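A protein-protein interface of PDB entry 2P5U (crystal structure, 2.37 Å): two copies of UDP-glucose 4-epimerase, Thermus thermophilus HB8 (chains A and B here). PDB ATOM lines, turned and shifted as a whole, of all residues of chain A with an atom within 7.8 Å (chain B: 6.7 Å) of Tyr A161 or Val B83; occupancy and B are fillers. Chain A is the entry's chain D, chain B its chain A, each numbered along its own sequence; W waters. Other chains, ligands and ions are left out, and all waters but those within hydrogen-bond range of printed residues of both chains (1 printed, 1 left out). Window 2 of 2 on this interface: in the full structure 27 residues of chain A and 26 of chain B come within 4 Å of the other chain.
No position is printed for both chains. Of the 11 pairs that touch across the chains among the printed residues, none has its exchanged pair printed and touching as well.
Water W1 lies within hydrogen-bond range of OG of Ser A160 (2.5 Å), O of Lys B140 (3.3 Å) and N of Gly B273 (3.3 Å).
The backbone carbonyl oxygen (O) of Val B83 sits at hydrogen-bond distance from the side-chain hydroxyl (OH) of Tyr A161 (2.7 Å). The backbone carbonyl oxygen of Lys B140 lies within hydrogen-bond range of the side-chain hydroxyl of Ser A160, 3.1 Å away.
OG of Ser B82 lies within hydrogen-bond range of O of Val B79 (2.8 Å). The backbone NH (N) of Tyr B143 sits at hydrogen-bond distance from the side-chain hydroxyl (OG) of Ser B82 (3.0 Å). The backbone carbonyl oxygen (O) of Asp B274 sits at hydrogen-bond distance from the side-chain amino group (NZ) of Lys B140 (2.7 Å). The side-chain carboxylate of Glu A102 sits at hydrogen-bond distance from the side-chain hydroxyl of Tyr A157, at 2.8 Å. The backbone carbonyl oxygen (O) of Tyr A157 lies within hydrogen-bond range of the backbone NH (N) of Gly A162 (3.3 Å). N of Leu A163 is in hydrogen-bond range of O of Tyr A157 (3.4 Å).
Among the printed residues, pairs that only touch across the chains: Arg A105 with Pro B86 (3.4 Å), Val A156 with Ser B141 (3.4 Å), Tyr A157 with Pro B86 (3.5 Å), Val A156 with Lys B140 (3.5 Å), Gln A159 with Lys B140 (3.6 Å), Glu A102 with Pro B86 (3.6 Å), Tyr A161 with Pro B86 (3.7 Å), Tyr A161 with Ser B82 (3.8 Å) and Tyr A153 with Pro B142 (3.996 Å).
Printed residues of chain B that touch a printed residue of chain A: Ser B82, Val B83, Pro B86, Lys B140, Ser B141 and Pro B142. Printed residues of chain A that touch a printed residue of chain B: Glu A102, Arg A105, Tyr A153, Val A156, Tyr A157, Gln A159, Ser A160 and Tyr A161. Hydrophobic or aromatic side chains of chain A within 4 Å of the printed part of chain B: Tyr A153, Val A156, Tyr A157 and Tyr A161. Among the printed residues, no Asp or Glu carboxylate lies within 4 Å of a Lys or Arg side-chain nitrogen of the other chain.
Of the printed residues of chain B, Glu A102 touches Pro B86. Of the printed residues of chain B, Val A156 touches Lys B140 and Ser B141. Of the printed residues of chain B, Tyr A161 touches Ser B82 (3.8 Å), Val B83 (2.7 Å) and Pro B86 (3.7 Å). Gln B76 touches none of the printed residues of chain A. Ser B82 touches just one residue of chain A: Tyr A161. Asp B85 touches none of the printed residues of chain A. Of the printed residues of chain A, Ser B141 touches Val A156 (3.4 Å). The nearest printed residue of chain B that does not touch Tyr A157 is Pro B142 (5.3 Å).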
ATOM      1  N   LEU A 101      -8.550   5.248  -8.187  1.00  0.00           N
ATOM      2  CA  LEU A 101      -8.456   5.292  -6.736  1.00  0.00           C
ATOM      3  C   LEU A 101      -8.224   6.729  -6.271  1.00  0.00           C
ATOM      4  O   LEU A 101      -8.820   7.179  -5.289  1.00  0.00           O
ATOM      5  CB  LEU A 101      -7.313   4.378  -6.272  1.00  0.00           C
ATOM      6  CG  LEU A 101      -7.615   3.084  -5.515  1.00  0.00           C
ATOM      7  CD1 LEU A 101      -8.894   2.421  -6.002  1.00  0.00           C
ATOM      8  CD2 LEU A 101      -6.424   2.143  -5.682  1.00  0.00           C
ATOM      9  N   GLU A 102      -7.357   7.454  -6.970  1.00  0.00           N
ATOM     10  CA  GLU A 102      -7.090   8.843  -6.600  1.00  0.00           C
ATOM     11  C   GLU A 102      -8.359   9.679  -6.725  1.00  0.00           C
ATOM     12  O   GLU A 102      -8.602  10.585  -5.927  1.00  0.00           O
ATOM     13  CB  GLU A 102      -5.989   9.440  -7.480  1.00  0.00           C
ATOM     14  CG  GLU A 102      -4.580   9.114  -7.009  1.00  0.00           C
ATOM     15  CD  GLU A 102      -4.260   9.728  -5.655  1.00  0.00           C
ATOM     16  OE1 GLU A 102      -4.592   9.117  -4.610  1.00  0.00           O
ATOM     17  OE2 GLU A 102      -3.685  10.841  -5.636  1.00  0.00           O
ATOM     18  N   CYS A 104     -11.362   8.479  -6.398  1.00  0.00           N
ATOM     19  CA  CYS A 104     -12.225   8.067  -5.298  1.00  0.00           C
ATOM     20  C   CYS A 104     -11.865   8.816  -4.033  1.00  0.00           C
ATOM     21  O   CYS A 104     -12.738   9.244  -3.288  1.00  0.00           O
ATOM     22  CB  CYS A 104     -12.093   6.566  -5.049  1.00  0.00           C
ATOM     23  SG  CYS A 104     -12.856   5.564  -6.322  1.00  0.00           S
ATOM     24  N   ARG A 105     -10.567   8.966  -3.799  1.00  0.00           N
ATOM     25  CA  ARG A 105     -10.085   9.657  -2.615  1.00  0.00           C
ATOM     26  C   ARG A 105     -10.452  11.130  -2.666  1.00  0.00           C
ATOM     27  O   ARG A 105     -11.023  11.671  -1.725  1.00  0.00           O
ATOM     28  CB  ARG A 105      -8.569   9.523  -2.501  1.00  0.00           C
ATOM     29  CG  ARG A 105      -8.113   8.964  -1.176  1.00  0.00           C
ATOM     30  CD  ARG A 105      -6.920   9.729  -0.638  1.00  0.00           C
ATOM     31  NE  ARG A 105      -5.891   9.887  -1.648  1.00  0.00           N
ATOM     32  CZ  ARG A 105      -4.768  10.570  -1.465  1.00  0.00           C
ATOM     33  NH1 ARG A 105      -4.529  11.155  -0.297  1.00  0.00           N
ATOM     34  NH2 ARG A 105      -3.893  10.683  -2.458  1.00  0.00           N
ATOM     35  N   VAL A 109     -15.354   8.959  -2.251  1.00  0.00           N
ATOM     36  CA  VAL A 109     -16.194   7.807  -2.562  1.00  0.00           C
ATOM     37  C   VAL A 109     -16.265   6.939  -1.301  1.00  0.00           C
ATOM     38  O   VAL A 109     -15.294   6.845  -0.558  1.00  0.00           O
ATOM     39  CB  VAL A 109     -15.585   6.986  -3.719  1.00  0.00           C
ATOM     40  CG1 VAL A 109     -16.296   5.655  -3.860  1.00  0.00           C
ATOM     41  CG2 VAL A 109     -15.683   7.782  -5.012  1.00  0.00           C
ATOM     42  N   TYR A 153      -3.057  -2.191  -3.418  1.00  0.00           N
ATOM     43  CA  TYR A 153      -3.372  -0.778  -3.367  1.00  0.00           C
ATOM     44  C   TYR A 153      -4.716  -0.534  -2.683  1.00  0.00           C
ATOM     45  O   TYR A 153      -4.850   0.384  -1.867  1.00  0.00           O
ATOM     46  CB  TYR A 153      -3.317  -0.194  -4.776  1.00  0.00           C
ATOM     47  CG  TYR A 153      -1.916   0.280  -5.110  1.00  0.00           C
ATOM     48  CD1 TYR A 153      -1.440   1.498  -4.621  1.00  0.00           C
ATOM     49  CD2 TYR A 153      -1.050  -0.508  -5.867  1.00  0.00           C
ATOM     50  CE1 TYR A 153      -0.142   1.921  -4.881  1.00  0.00           C
ATOM     51  CE2 TYR A 153       0.256  -0.091  -6.129  1.00  0.00           C
ATOM     52  CZ  TYR A 153       0.696   1.123  -5.634  1.00  0.00           C
ATOM     53  OH  TYR A 153       1.961   1.557  -5.916  1.00  0.00           O
ATOM     54  N   LEU A 154      -5.707  -1.367  -2.988  1.00  0.00           N
ATOM     55  CA  LEU A 154      -7.004  -1.217  -2.340  1.00  0.00           C
ATOM     56  C   LEU A 154      -6.833  -1.320  -0.822  1.00  0.00           C
ATOM     57  O   LEU A 154      -7.363  -0.501  -0.079  1.00  0.00           O
ATOM     58  CB  LEU A 154      -7.973  -2.302  -2.809  1.00  0.00           C
ATOM     59  CG  LEU A 154      -8.636  -2.095  -4.164  1.00  0.00           C
ATOM     60  CD1 LEU A 154      -9.242  -3.415  -4.628  1.00  0.00           C
ATOM     61  CD2 LEU A 154      -9.705  -1.002  -4.057  1.00  0.00           C
ATOM     62  N   SER A 155      -6.092  -2.330  -0.367  1.00  0.00           N
ATOM     63  CA  SER A 155      -5.875  -2.518   1.067  1.00  0.00           C
ATOM     64  C   SER A 155      -5.151  -1.340   1.727  1.00  0.00           C
ATOM     65  O   SER A 155      -5.515  -0.941   2.834  1.00  0.00           O
ATOM     66  CB  SER A 155      -5.092  -3.806   1.327  1.00  0.00           C
ATOM     67  OG  SER A 155      -4.681  -3.878   2.693  1.00  0.00           O
ATOM     68  N   VAL A 156      -4.132  -0.784   1.066  1.00  0.00           N
ATOM     69  CA  VAL A 156      -3.416   0.350   1.653  1.00  0.00           C
ATOM     70  C   VAL A 156      -4.256   1.625   1.596  1.00  0.00           C
ATOM     71  O   VAL A 156      -4.173   2.468   2.490  1.00  0.00           O
ATOM     72  CB  VAL A 156      -2.027   0.612   0.982  1.00  0.00           C
ATOM     73  CG1 VAL A 156      -1.114  -0.589   1.189  1.00  0.00           C
ATOM     74  CG2 VAL A 156      -2.199   0.912  -0.495  1.00  0.00           C
ATOM     75  N   TYR A 157      -5.064   1.775   0.551  1.00  0.00           N
ATOM     76  CA  TYR A 157      -5.922   2.953   0.465  1.00  0.00           C
ATOM     77  C   TYR A 157      -6.980   2.844   1.554  1.00  0.00           C
ATOM     78  O   TYR A 157      -7.447   3.851   2.084  1.00  0.00           O
ATOM     79  CB  TYR A 157      -6.589   3.060  -0.908  1.00  0.00           C
ATOM     80  CG  TYR A 157      -5.828   3.953  -1.860  1.00  0.00           C
ATOM     81  CD1 TYR A 157      -6.361   5.175  -2.285  1.00  0.00           C
ATOM     82  CD2 TYR A 157      -4.557   3.599  -2.307  1.00  0.00           C
ATOM     83  CE1 TYR A 157      -5.646   6.021  -3.135  1.00  0.00           C
ATOM     84  CE2 TYR A 157      -3.834   4.436  -3.154  1.00  0.00           C
ATOM     85  CZ  TYR A 157      -4.385   5.642  -3.561  1.00  0.00           C
ATOM     86  OH  TYR A 157      -3.671   6.452  -4.401  1.00  0.00           O
ATOM     87  N   GLY A 158      -7.344   1.612   1.894  1.00  0.00           N
ATOM     88  CA  GLY A 158      -8.321   1.416   2.945  1.00  0.00           C
ATOM     89  C   GLY A 158      -7.712   1.799   4.283  1.00  0.00           C
ATOM     90  O   GLY A 158      -8.304   2.549   5.058  1.00  0.00           O
ATOM     91  N   GLN A 159      -6.510   1.298   4.552  1.00  0.00           N
ATOM     92  CA  GLN A 159      -5.825   1.578   5.813  1.00  0.00           C
ATOM     93  C   GLN A 159      -5.329   3.017   5.958  1.00  0.00           C
ATOM     94  O   GLN A 159      -5.353   3.569   7.063  1.00  0.00           O
ATOM     95  CB  GLN A 159      -4.626   0.639   5.986  1.00  0.00           C
ATOM     96  CG  GLN A 159      -4.964  -0.829   6.211  1.00  0.00           C
ATOM     97  CD  GLN A 159      -3.735  -1.718   6.051  1.00  0.00           C
ATOM     98  OE1 GLN A 159      -3.442  -2.208   4.959  1.00  0.00           O
ATOM     99  NE2 GLN A 159      -3.008  -1.918   7.141  1.00  0.00           N
ATOM    100  N   SER A 160      -4.872   3.613   4.856  1.00  0.00           N
ATOM    101  CA  SER A 160      -4.329   4.977   4.878  1.00  0.00           C
ATOM    102  C   SER A 160      -5.323   6.112   4.678  1.00  0.00           C
ATOM    103  O   SER A 160      -5.190   7.170   5.292  1.00  0.00           O
ATOM    104  CB  SER A 160      -3.243   5.138   3.812  1.00  0.00           C
ATOM    105  OG  SER A 160      -2.211   4.182   3.964  1.00  0.00           O
ATOM    106  N   TYR A 161      -6.309   5.910   3.815  1.00  0.00           N
ATOM    107  CA  TYR A 161      -7.267   6.970   3.534  1.00  0.00           C
ATOM    108  C   TYR A 161      -8.720   6.666   3.855  1.00  0.00           C
ATOM    109  O   TYR A 161      -9.594   7.448   3.499  1.00  0.00           O
ATOM    110  CB  TYR A 161      -7.162   7.370   2.067  1.00  0.00           C
ATOM    111  CG  TYR A 161      -5.737   7.527   1.606  1.00  0.00           C
ATOM    112  CD1 TYR A 161      -4.893   8.473   2.196  1.00  0.00           C
ATOM    113  CD2 TYR A 161      -5.221   6.701   0.604  1.00  0.00           C
ATOM    114  CE1 TYR A 161      -3.566   8.590   1.799  1.00  0.00           C
ATOM    115  CE2 TYR A 161      -3.903   6.806   0.199  1.00  0.00           C
ATOM    116  CZ  TYR A 161      -3.078   7.755   0.805  1.00  0.00           C
ATOM    117  OH  TYR A 161      -1.769   7.857   0.411  1.00  0.00           O
ATOM    118  N   GLY A 162      -8.985   5.534   4.498  1.00  0.00           N
ATOM    119  CA  GLY A 162     -10.356   5.208   4.856  1.00  0.00           C
ATOM    120  C   GLY A 162     -11.299   4.756   3.752  1.00  0.00           C
ATOM    121  O   GLY A 162     -12.507   4.699   3.967  1.00  0.00           O
ATOM    122  N   LEU A 163     -10.781   4.441   2.570  1.00  0.00           N
ATOM    123  CA  LEU A 163     -11.643   3.977   1.477  1.00  0.00           C
ATOM    124  C   LEU A 163     -12.107   2.529   1.723  1.00  0.00           C
ATOM    125  O   LEU A 163     -11.277   1.639   1.889  1.00  0.00           O
ATOM    126  CB  LEU A 163     -10.880   4.046   0.150  1.00  0.00           C
ATOM    127  CG  LEU A 163     -11.593   3.419  -1.051  1.00  0.00           C
ATOM    128  CD1 LEU A 163     -12.867   4.204  -1.348  1.00  0.00           C
ATOM    129  CD2 LEU A 163     -10.673   3.418  -2.269  1.00  0.00           C
ATOM    130  N   LYS A 164     -13.418   2.288   1.757  1.00  0.00           N
ATOM    131  CA  LYS A 164     -13.916   0.926   1.968  1.00  0.00           C
ATOM    132  C   LYS A 164     -13.813   0.154   0.652  1.00  0.00           C
ATOM    133  O   LYS A 164     -14.096   0.691  -0.420  1.00  0.00           O
ATOM    134  CB  LYS A 164     -15.370   0.932   2.433  1.00  0.00           C
ATOM    135  CG  LYS A 164     -15.592   1.529   3.809  1.00  0.00           C
ATOM    136  CD  LYS A 164     -17.068   1.446   4.191  1.00  0.00           C
ATOM    137  CE  LYS A 164     -17.351   2.140   5.524  1.00  0.00           C
ATOM    138  NZ  LYS A 164     -16.454   1.659   6.617  1.00  0.00           N
ATOM    139  N   GLN B  76      11.514   5.456  -4.658  1.00  0.00           N
ATOM    140  CA  GLN B  76      11.055   6.497  -3.760  1.00  0.00           C
ATOM    141  C   GLN B  76      11.099   5.710  -2.451  1.00  0.00           C
ATOM    142  O   GLN B  76      10.257   4.842  -2.206  1.00  0.00           O
ATOM    143  CB  GLN B  76       9.623   6.907  -4.115  1.00  0.00           C
ATOM    144  CG  GLN B  76       9.117   8.135  -3.381  1.00  0.00           C
ATOM    145  CD  GLN B  76       8.846   7.868  -1.911  1.00  0.00           C
ATOM    146  OE1 GLN B  76       7.970   7.074  -1.568  1.00  0.00           O
ATOM    147  NE2 GLN B  76       9.602   8.525  -1.036  1.00  0.00           N
ATOM    148  N   SER B  78      10.524   6.167   0.972  1.00  0.00           N
ATOM    149  CA  SER B  78       9.978   6.858   2.131  1.00  0.00           C
ATOM    150  C   SER B  78       8.501   6.586   2.342  1.00  0.00           C
ATOM    151  O   SER B  78       7.664   6.955   1.509  1.00  0.00           O
ATOM    152  CB  SER B  78      10.200   8.365   2.017  1.00  0.00           C
ATOM    153  OG  SER B  78       9.575   9.033   3.107  1.00  0.00           O
ATOM    154  N   VAL B  79       8.189   5.938   3.462  1.00  0.00           N
ATOM    155  CA  VAL B  79       6.810   5.623   3.805  1.00  0.00           C
ATOM    156  C   VAL B  79       5.970   6.898   3.884  1.00  0.00           C
ATOM    157  O   VAL B  79       4.891   6.975   3.288  1.00  0.00           O
ATOM    158  CB  VAL B  79       6.734   4.864   5.155  1.00  0.00           C
ATOM    159  CG1 VAL B  79       5.295   4.800   5.648  1.00  0.00           C
ATOM    160  CG2 VAL B  79       7.287   3.447   4.979  1.00  0.00           C
ATOM    161  N   LYS B  80       6.480   7.900   4.599  1.00  0.00           N
ATOM    162  CA  LYS B  80       5.786   9.174   4.770  1.00  0.00           C
ATOM    163  C   LYS B  80       5.473   9.837   3.428  1.00  0.00           C
ATOM    164  O   LYS B  80       4.339  10.254   3.177  1.00  0.00           O
ATOM    165  CB  LYS B  80       6.628  10.125   5.628  1.00  0.00           C
ATOM    166  CG  LYS B  80       5.915  11.422   6.004  1.00  0.00           C
ATOM    167  CD  LYS B  80       6.852  12.410   6.695  1.00  0.00           C
ATOM    168  CE  LYS B  80       6.119  13.705   7.035  1.00  0.00           C
ATOM    169  NZ  LYS B  80       7.039  14.781   7.506  1.00  0.00           N
ATOM    170  N   VAL B  81       6.481   9.941   2.570  1.00  0.00           N
ATOM    171  CA  VAL B  81       6.290  10.543   1.256  1.00  0.00           C
ATOM    172  C   VAL B  81       5.261   9.750   0.449  1.00  0.00           C
ATOM    173  O   VAL B  81       4.445  10.337  -0.257  1.00  0.00           O
ATOM    174  CB  VAL B  81       7.633  10.622   0.459  1.00  0.00           C
ATOM    175  CG1 VAL B  81       7.381  11.124  -0.961  1.00  0.00           C
ATOM    176  CG2 VAL B  81       8.603  11.577   1.164  1.00  0.00           C
ATOM    177  N   SER B  82       5.278   8.421   0.565  1.00  0.00           N
ATOM    178  CA  SER B  82       4.327   7.608  -0.188  1.00  0.00           C
ATOM    179  C   SER B  82       2.894   7.831   0.288  1.00  0.00           C
ATOM    180  O   SER B  82       1.957   7.758  -0.510  1.00  0.00           O
ATOM    181  CB  SER B  82       4.684   6.118  -0.105  1.00  0.00           C
ATOM    182  OG  SER B  82       4.145   5.512   1.056  1.00  0.00           O
ATOM    183  N   VAL B  83       2.718   8.093   1.583  1.00  0.00           N
ATOM    184  CA  VAL B  83       1.380   8.344   2.129  1.00  0.00           C
ATOM    185  C   VAL B  83       0.895   9.724   1.686  1.00  0.00           C
ATOM    186  O   VAL B  83      -0.275   9.905   1.360  1.00  0.00           O
ATOM    187  CB  VAL B  83       1.351   8.327   3.684  1.00  0.00           C
ATOM    188  CG1 VAL B  83      -0.048   8.723   4.181  1.00  0.00           C
ATOM    189  CG2 VAL B  83       1.728   6.942   4.212  1.00  0.00           C
ATOM    190  N   GLU B  84       1.797  10.697   1.665  1.00  0.00           N
ATOM    191  CA  GLU B  84       1.418  12.043   1.263  1.00  0.00           C
ATOM    192  C   GLU B  84       1.283  12.168  -0.249  1.00  0.00           C
ATOM    193  O   GLU B  84       0.465  12.941  -0.740  1.00  0.00           O
ATOM    194  CB  GLU B  84       2.443  13.056   1.783  1.00  0.00           C
ATOM    195  CG  GLU B  84       2.616  13.013   3.301  1.00  0.00           C
ATOM    196  CD  GLU B  84       3.705  13.951   3.814  1.00  0.00           C
ATOM    197  OE1 GLU B  84       4.758  14.083   3.135  1.00  0.00           O
ATOM    198  OE2 GLU B  84       3.518  14.533   4.913  1.00  0.00           O
ATOM    199  N   ASP B  85       2.058  11.382  -0.989  1.00  0.00           N
ATOM    200  CA  ASP B  85       2.031  11.451  -2.449  1.00  0.00           C
ATOM    201  C   ASP B  85       2.101  10.046  -3.065  1.00  0.00           C
ATOM    202  O   ASP B  85       3.133   9.637  -3.602  1.00  0.00           O
ATOM    203  CB  ASP B  85       3.220  12.315  -2.898  1.00  0.00           C
ATOM    204  CG  ASP B  85       3.186  12.659  -4.375  1.00  0.00           C
ATOM    205  OD1 ASP B  85       4.065  13.435  -4.805  1.00  0.00           O
ATOM    206  OD2 ASP B  85       2.299  12.163  -5.104  1.00  0.00           O
ATOM    207  N   PRO B  86       0.988   9.298  -3.013  1.00  0.00           N
ATOM    208  CA  PRO B  86       0.952   7.940  -3.561  1.00  0.00           C
ATOM    209  C   PRO B  86       1.263   7.842  -5.051  1.00  0.00           C
ATOM    210  O   PRO B  86       1.860   6.866  -5.509  1.00  0.00           O
ATOM    211  CB  PRO B  86      -0.455   7.457  -3.201  1.00  0.00           C
ATOM    212  CG  PRO B  86      -1.257   8.717  -3.202  1.00  0.00           C
ATOM    213  CD  PRO B  86      -0.339   9.704  -2.516  1.00  0.00           C
ATOM    214  N   ASP B  89       5.059   7.783  -5.576  1.00  0.00           N
ATOM    215  CA  ASP B  89       5.651   6.499  -5.199  1.00  0.00           C
ATOM    216  C   ASP B  89       5.389   5.456  -6.296  1.00  0.00           C
ATOM    217  O   ASP B  89       6.271   4.676  -6.659  1.00  0.00           O
ATOM    218  CB  ASP B  89       5.052   6.002  -3.884  1.00  0.00           C
ATOM    219  CG  ASP B  89       5.569   4.637  -3.499  1.00  0.00           C
ATOM    220  OD1 ASP B  89       6.740   4.550  -3.069  1.00  0.00           O
ATOM    221  OD2 ASP B  89       4.811   3.646  -3.640  1.00  0.00           O
ATOM    222  N   LYS B 140       0.760  -1.758   4.349  1.00  0.00           N
ATOM    223  CA  LYS B 140      -0.098  -0.784   5.015  1.00  0.00           C
ATOM    224  C   LYS B 140      -0.016   0.576   4.329  1.00  0.00           C
ATOM    225  O   LYS B 140      -0.982   1.334   4.319  1.00  0.00           O
ATOM    226  CB  LYS B 140       0.320  -0.617   6.473  1.00  0.00           C
ATOM    227  CG  LYS B 140      -0.387   0.529   7.172  1.00  0.00           C
ATOM    228  CD  LYS B 140       0.022   0.593   8.632  1.00  0.00           C
ATOM    229  CE  LYS B 140      -0.702   1.697   9.371  1.00  0.00           C
ATOM    230  NZ  LYS B 140      -0.268   1.695  10.788  1.00  0.00           N
ATOM    231  N   SER B 141       1.151   0.879   3.772  1.00  0.00           N
ATOM    232  CA  SER B 141       1.394   2.145   3.087  1.00  0.00           C
ATOM    233  C   SER B 141       1.598   1.920   1.586  1.00  0.00           C
ATOM    234  O   SER B 141       1.991   0.834   1.167  1.00  0.00           O
ATOM    235  CB  SER B 141       2.631   2.812   3.684  1.00  0.00           C
ATOM    236  OG  SER B 141       3.775   1.985   3.549  1.00  0.00           O
ATOM    237  N   PRO B 142       1.332   2.942   0.756  1.00  0.00           N
ATOM    238  CA  PRO B 142       1.507   2.772  -0.694  1.00  0.00           C
ATOM    239  C   PRO B 142       2.921   2.380  -1.089  1.00  0.00           C
ATOM    240  O   PRO B 142       3.143   1.712  -2.102  1.00  0.00           O
ATOM    241  CB  PRO B 142       1.064   4.121  -1.276  1.00  0.00           C
ATOM    242  CG  PRO B 142       1.045   5.059  -0.117  1.00  0.00           C
ATOM    243  CD  PRO B 142       0.690   4.230   1.071  1.00  0.00           C
ATOM    244  N   TYR B 143       3.874   2.791  -0.271  1.00  0.00           N
ATOM    245  CA  TYR B 143       5.249   2.447  -0.517  1.00  0.00           C
ATOM    246  C   TYR B 143       5.390   0.921  -0.454  1.00  0.00           C
ATOM    247  O   TYR B 143       5.961   0.310  -1.348  1.00  0.00           O
ATOM    248  CB  TYR B 143       6.125   3.103   0.533  1.00  0.00           C
ATOM    249  CG  TYR B 143       7.493   2.503   0.619  1.00  0.00           C
ATOM    250  CD1 TYR B 143       7.799   1.593   1.624  1.00  0.00           C
ATOM    251  CD2 TYR B 143       8.492   2.866  -0.278  1.00  0.00           C
ATOM    252  CE1 TYR B 143       9.070   1.065   1.749  1.00  0.00           C
ATOM    253  CE2 TYR B 143       9.774   2.336  -0.165  1.00  0.00           C
ATOM    254  CZ  TYR B 143      10.048   1.442   0.860  1.00  0.00           C
ATOM    255  OH  TYR B 143      11.321   0.961   1.036  1.00  0.00           O
ATOM    256  N   PRO B 272       1.502   8.737   9.981  1.00  0.00           N
ATOM    257  CA  PRO B 272       0.753   7.861   9.077  1.00  0.00           C
ATOM    258  C   PRO B 272       1.602   6.943   8.198  1.00  0.00           C
ATOM    259  O   PRO B 272       2.626   7.349   7.641  1.00  0.00           O
ATOM    260  CB  PRO B 272      -0.077   8.848   8.258  1.00  0.00           C
ATOM    261  CG  PRO B 272       0.822  10.035   8.172  1.00  0.00           C
ATOM    262  CD  PRO B 272       1.311  10.152   9.604  1.00  0.00           C
ATOM    263  N   GLY B 273       1.148   5.703   8.085  1.00  0.00           N
ATOM    264  CA  GLY B 273       1.843   4.729   7.275  1.00  0.00           C
ATOM    265  C   GLY B 273       2.758   3.818   8.063  1.00  0.00           C
ATOM    266  O   GLY B 273       3.050   2.713   7.613  1.00  0.00           O
ATOM    267  N   ASP B 274       3.217   4.265   9.230  1.00  0.00           N
ATOM    268  CA  ASP B 274       4.122   3.454  10.043  1.00  0.00           C
ATOM    269  C   ASP B 274       3.483   2.256  10.725  1.00  0.00           C
ATOM    270  O   ASP B 274       2.340   2.316  11.178  1.00  0.00           O
ATOM    271  CB  ASP B 274       4.787   4.291  11.141  1.00  0.00           C
ATOM    272  CG  ASP B 274       6.070   4.962  10.681  1.00  0.00           C
ATOM    273  OD1 ASP B 274       6.639   4.536   9.643  1.00  0.00           O
ATOM    274  OD2 ASP B 274       6.515   5.905  11.379  1.00  0.00           O
HETATM  275  O   HOH W   1      -1.004   4.044   6.127  1.00  0.00           O
